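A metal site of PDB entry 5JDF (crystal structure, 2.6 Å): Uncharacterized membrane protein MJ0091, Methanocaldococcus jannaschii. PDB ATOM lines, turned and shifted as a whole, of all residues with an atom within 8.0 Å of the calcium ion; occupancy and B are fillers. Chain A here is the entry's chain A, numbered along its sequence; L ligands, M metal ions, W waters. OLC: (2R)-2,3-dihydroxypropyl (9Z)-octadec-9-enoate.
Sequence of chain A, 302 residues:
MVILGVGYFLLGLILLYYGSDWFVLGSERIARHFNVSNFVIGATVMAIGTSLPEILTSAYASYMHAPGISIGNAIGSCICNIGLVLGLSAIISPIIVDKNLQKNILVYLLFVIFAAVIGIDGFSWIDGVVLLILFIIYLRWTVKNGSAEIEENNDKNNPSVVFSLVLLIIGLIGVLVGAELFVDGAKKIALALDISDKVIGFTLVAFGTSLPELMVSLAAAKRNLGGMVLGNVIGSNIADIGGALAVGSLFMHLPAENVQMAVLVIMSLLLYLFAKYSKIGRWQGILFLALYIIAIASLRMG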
ATOM      1  N   ALA A 115      -9.547   6.551  19.615  1.00  0.00           N
ATOM      2  CA  ALA A 115      -8.339   6.536  20.430  1.00  0.00           C
ATOM      3  C   ALA A 115      -8.668   6.307  21.895  1.00  0.00           C
ATOM      4  O   ALA A 115      -7.965   5.577  22.600  1.00  0.00           O
ATOM      5  CB  ALA A 115      -7.570   7.834  20.261  1.00  0.00           C
ATOM      6  N   ALA A 116      -9.759   6.924  22.352  1.00  0.00           N
ATOM      7  CA  ALA A 116     -10.179   6.827  23.742  1.00  0.00           C
ATOM      8  C   ALA A 116     -10.591   5.404  24.103  1.00  0.00           C
ATOM      9  O   ALA A 116     -10.289   4.924  25.196  1.00  0.00           O
ATOM     10  CB  ALA A 116     -11.309   7.796  24.009  1.00  0.00           C
ATOM     11  N   VAL A 117     -11.286   4.736  23.178  1.00  0.00           N
ATOM     12  CA  VAL A 117     -11.756   3.383  23.415  1.00  0.00           C
ATOM     13  C   VAL A 117     -10.609   2.379  23.523  1.00  0.00           C
ATOM     14  O   VAL A 117     -10.555   1.579  24.457  1.00  0.00           O
ATOM     15  CB  VAL A 117     -12.710   2.924  22.291  1.00  0.00           C
ATOM     16  CG1 VAL A 117     -12.977   1.433  22.383  1.00  0.00           C
ATOM     17  CG2 VAL A 117     -14.020   3.711  22.343  1.00  0.00           C
ATOM     18  N   ILE A 118      -9.677   2.442  22.576  1.00  0.00           N
ATOM     19  CA  ILE A 118      -8.558   1.508  22.550  1.00  0.00           C
ATOM     20  C   ILE A 118      -7.509   1.848  23.603  1.00  0.00           C
ATOM     21  O   ILE A 118      -6.540   1.120  23.784  1.00  0.00           O
ATOM     22  CB  ILE A 118      -7.878   1.472  21.161  1.00  0.00           C
ATOM     23  CG1 ILE A 118      -7.082   2.753  20.924  1.00  0.00           C
ATOM     24  CG2 ILE A 118      -8.912   1.248  20.073  1.00  0.00           C
ATOM     25  CD1 ILE A 118      -6.247   2.728  19.668  1.00  0.00           C
ATOM     26  N   GLY A 119      -7.708   2.962  24.302  1.00  0.00           N
ATOM     27  CA  GLY A 119      -6.765   3.412  25.303  1.00  0.00           C
ATOM     28  C   GLY A 119      -7.180   3.138  26.737  1.00  0.00           C
ATOM     29  O   GLY A 119      -6.443   3.413  27.673  1.00  0.00           O
ATOM     30  N   ILE A 120      -8.386   2.583  26.898  1.00  0.00           N
ATOM     31  CA  ILE A 120      -8.934   2.261  28.210  1.00  0.00           C
ATOM     32  C   ILE A 120      -8.004   1.342  29.002  1.00  0.00           C
ATOM     33  O   ILE A 120      -7.817   1.521  30.205  1.00  0.00           O
ATOM     34  CB  ILE A 120     -10.310   1.585  28.076  1.00  0.00           C
ATOM     35  CG1 ILE A 120     -11.294   2.517  27.369  1.00  0.00           C
ATOM     36  CG2 ILE A 120     -10.851   1.196  29.447  1.00  0.00           C
ATOM     37  CD1 ILE A 120     -12.655   1.897  27.133  1.00  0.00           C
ATOM     38  N   ASP A 121      -7.427   0.365  28.319  1.00  0.00           N
ATOM     39  CA  ASP A 121      -6.483  -0.558  28.941  1.00  0.00           C
ATOM     40  C   ASP A 121      -5.054  -0.103  28.699  1.00  0.00           C
ATOM     41  O   ASP A 121      -4.108  -0.880  28.856  1.00  0.00           O
ATOM     42  CB  ASP A 121      -6.687  -1.979  28.406  1.00  0.00           C
ATOM     43  CG  ASP A 121      -6.710  -2.028  26.888  1.00  0.00           C
ATOM     44  OD1 ASP A 121      -7.096  -1.020  26.263  1.00  0.00           O
ATOM     45  OD2 ASP A 121      -6.352  -3.083  26.329  1.00  0.00           O
ATOM     46  N   GLY A 122      -4.893   1.156  28.318  1.00  0.00           N
ATOM     47  CA  GLY A 122      -3.596   1.703  27.997  1.00  0.00           C
ATOM     48  C   GLY A 122      -3.351   1.725  26.497  1.00  0.00           C
ATOM     49  O   GLY A 122      -4.258   1.424  25.722  1.00  0.00           O
ATOM     50  N   PHE A 123      -2.141   2.080  26.096  1.00  0.00           N
ATOM     51  CA  PHE A 123      -1.789   2.124  24.683  1.00  0.00           C
ATOM     52  C   PHE A 123      -0.604   1.220  24.365  1.00  0.00           C
ATOM     53  O   PHE A 123       0.547   1.575  24.649  1.00  0.00           O
ATOM     54  CB  PHE A 123      -1.488   3.556  24.232  1.00  0.00           C
ATOM     55  CG  PHE A 123      -2.703   4.435  24.163  1.00  0.00           C
ATOM     56  CD1 PHE A 123      -3.511   4.428  23.037  1.00  0.00           C
ATOM     57  CD2 PHE A 123      -3.024   5.282  25.211  1.00  0.00           C
ATOM     58  CE1 PHE A 123      -4.617   5.247  22.967  1.00  0.00           C
ATOM     59  CE2 PHE A 123      -4.138   6.098  25.145  1.00  0.00           C
ATOM     60  CZ  PHE A 123      -4.941   6.078  24.018  1.00  0.00           C
ATOM     61  N   SER A 124      -0.892   0.057  23.798  1.00  0.00           N
ATOM     62  CA  SER A 124       0.157  -0.858  23.363  1.00  0.00           C
ATOM     63  C   SER A 124       0.860  -0.300  22.148  1.00  0.00           C
ATOM     64  O   SER A 124       0.380   0.651  21.518  1.00  0.00           O
ATOM     65  CB  SER A 124      -0.427  -2.245  23.056  1.00  0.00           C
ATOM     66  OG  SER A 124      -1.304  -2.190  21.946  1.00  0.00           O
ATOM     67  N   TRP A 125       2.013  -0.877  21.800  1.00  0.00           N
ATOM     68  CA  TRP A 125       2.744  -0.456  20.615  1.00  0.00           C
ATOM     69  C   TRP A 125       1.899  -0.676  19.363  1.00  0.00           C
ATOM     70  O   TRP A 125       2.025   0.051  18.389  1.00  0.00           O
ATOM     71  CB  TRP A 125       4.072  -1.209  20.500  1.00  0.00           C
ATOM     72  CG  TRP A 125       3.916  -2.691  20.386  1.00  0.00           C
ATOM     73  CD1 TRP A 125       3.815  -3.580  21.416  1.00  0.00           C
ATOM     74  CD2 TRP A 125       3.844  -3.461  19.180  1.00  0.00           C
ATOM     75  NE1 TRP A 125       3.679  -4.855  20.923  1.00  0.00           N
ATOM     76  CE2 TRP A 125       3.695  -4.807  19.552  1.00  0.00           C
ATOM     77  CE3 TRP A 125       3.886  -3.122  17.825  1.00  0.00           C
ATOM     78  CZ2 TRP A 125       3.600  -5.827  18.612  1.00  0.00           C
ATOM     79  CZ3 TRP A 125       3.782  -4.146  16.888  1.00  0.00           C
ATOM     80  CH2 TRP A 125       3.642  -5.482  17.293  1.00  0.00           C
ATOM     81  N   ILE A 126       1.031  -1.682  19.416  1.00  0.00           N
ATOM     82  CA  ILE A 126       0.106  -1.966  18.328  1.00  0.00           C
ATOM     83  C   ILE A 126      -0.935  -0.846  18.206  1.00  0.00           C
ATOM     84  O   ILE A 126      -1.263  -0.431  17.091  1.00  0.00           O
ATOM     85  CB  ILE A 126      -0.613  -3.313  18.538  1.00  0.00           C
ATOM     86  CG1 ILE A 126       0.390  -4.467  18.444  1.00  0.00           C
ATOM     87  CG2 ILE A 126      -1.720  -3.510  17.503  1.00  0.00           C
ATOM     88  CD1 ILE A 126      -0.231  -5.836  18.525  1.00  0.00           C
ATOM     89  N   ASP A 127      -1.431  -0.365  19.338  1.00  0.00           N
ATOM     90  CA  ASP A 127      -2.348   0.768  19.360  1.00  0.00           C
ATOM     91  C   ASP A 127      -1.726   1.963  18.659  1.00  0.00           C
ATOM     92  O   ASP A 127      -2.391   2.665  17.899  1.00  0.00           O
ATOM     93  CB  ASP A 127      -2.732   1.142  20.791  1.00  0.00           C
ATOM     94  CG  ASP A 127      -3.643   0.130  21.449  1.00  0.00           C
ATOM     95  OD1 ASP A 127      -4.252  -0.683  20.716  1.00  0.00           O
ATOM     96  OD2 ASP A 127      -3.759   0.157  22.687  1.00  0.00           O
ATOM     97  N   GLY A 128      -0.441   2.176  18.913  1.00  0.00           N
ATOM     98  CA  GLY A 128       0.287   3.276  18.307  1.00  0.00           C
ATOM     99  C   GLY A 128       0.439   3.141  16.807  1.00  0.00           C
ATOM    100  O   GLY A 128       0.341   4.118  16.077  1.00  0.00           O
ATOM    101  N   HIS A 253       4.635   0.570  26.735  1.00  0.00           N
ATOM    102  CA  HIS A 253       3.207   0.665  26.961  1.00  0.00           C
ATOM    103  C   HIS A 253       2.849   1.922  27.744  1.00  0.00           C
ATOM    104  O   HIS A 253       3.444   2.209  28.774  1.00  0.00           O
ATOM    105  CB  HIS A 253       2.693  -0.576  27.705  1.00  0.00           C
ATOM    106  CG  HIS A 253       1.210  -0.560  27.937  1.00  0.00           C
ATOM    107  ND1 HIS A 253       0.314  -1.053  27.031  1.00  0.00           N
ATOM    108  CD2 HIS A 253       0.486  -0.108  28.995  1.00  0.00           C
ATOM    109  CE1 HIS A 253      -0.915  -0.909  27.512  1.00  0.00           C
ATOM    110  NE2 HIS A 253      -0.834  -0.343  28.688  1.00  0.00           N
ATOM    111  N   LEU A 254       1.882   2.677  27.226  1.00  0.00           N
ATOM    112  CA  LEU A 254       1.439   3.900  27.877  1.00  0.00           C
ATOM    113  C   LEU A 254       0.299   3.613  28.842  1.00  0.00           C
ATOM    114  O   LEU A 254      -0.665   2.934  28.481  1.00  0.00           O
ATOM    115  CB  LEU A 254       1.012   4.942  26.847  1.00  0.00           C
ATOM    116  CG  LEU A 254       2.021   5.291  25.747  1.00  0.00           C
ATOM    117  CD1 LEU A 254       1.450   6.373  24.838  1.00  0.00           C
ATOM    118  CD2 LEU A 254       3.341   5.742  26.352  1.00  0.00           C
ATOM    119  N   ALA A 256      -3.080   4.067  31.066  1.00  0.00           N
ATOM    120  CA  ALA A 256      -4.389   4.589  30.683  1.00  0.00           C
ATOM    121  C   ALA A 256      -4.720   5.908  31.373  1.00  0.00           C
ATOM    122  O   ALA A 256      -4.650   6.010  32.604  1.00  0.00           O
ATOM    123  CB  ALA A 256      -5.473   3.558  30.982  1.00  0.00           C
HETATM  124  C8  OLC L   1     -15.819   3.547  17.010  1.00  0.00           C
HETATM  125  C24 OLC L   1      -7.175  -1.937  22.150  1.00  0.00           C
HETATM  126  C7  OLC L   1     -15.190   2.769  18.170  1.00  0.00           C
HETATM  127  C6  OLC L   1     -14.320   1.624  17.616  1.00  0.00           C
HETATM  128  C5  OLC L   1     -13.716   0.881  18.810  1.00  0.00           C
HETATM  129  C4  OLC L   1     -12.824  -0.281  18.349  1.00  0.00           C
HETATM  130  C3  OLC L   1     -12.276  -0.942  19.613  1.00  0.00           C
HETATM  131  C2  OLC L   1     -11.357  -2.119  19.287  1.00  0.00           C
HETATM  132  C21 OLC L   1      -9.210  -3.377  22.019  1.00  0.00           C
HETATM  133  C1  OLC L   1     -10.864  -2.699  20.620  1.00  0.00           C
HETATM  134  C22 OLC L   1      -7.690  -3.375  22.240  1.00  0.00           C
HETATM  135  O19 OLC L   1     -11.665  -2.973  21.510  1.00  0.00           O
HETATM  136  O25 OLC L   1      -5.760  -1.927  22.353  1.00  0.00           O
HETATM  137  O23 OLC L   1      -7.401  -3.905  23.533  1.00  0.00           O
HETATM  138  O20 OLC L   1      -9.513  -2.846  20.723  1.00  0.00           O
HETATM  139 CA    CA M   1      -5.109  -0.586  24.666  1.00  0.00          CA
HETATM  140  O   HOH W   1      -3.485  -2.373  24.667  1.00  0.00           O
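Within 4 Å of the calcium ion: Ile 118, Asp 121, Gly 122 and Asp 127.
The nearest printed residue that does not touch the calcium ion is Phe 123 (4.2 Å).
Water W1 lies within hydrogen-bond range of the side-chain carboxylate of Asp 121 (3.4 Å) and the side-chain hydroxyl of Ser 124 (3.5 Å).
The calcium ion is bound by O of Ile 118 (2.4 Å), water W1 (2.4 Å), O of Gly 122 (2.4 Å), OD2 of Asp 127 (2.5 Å), OD1 of Asp 121 (2.6 Å) and O25 of the ligand (2.8 Å).
The backbone carbonyl oxygen (O) of Asp 121 lies within hydrogen-bond range of a ring nitrogen (NE2) of His 253, 3.3 Å away.
The backbone NH (N) of Asp 127 sits at hydrogen-bond distance from the side-chain hydroxyl (OG) of Ser 124 (3.2 Å).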
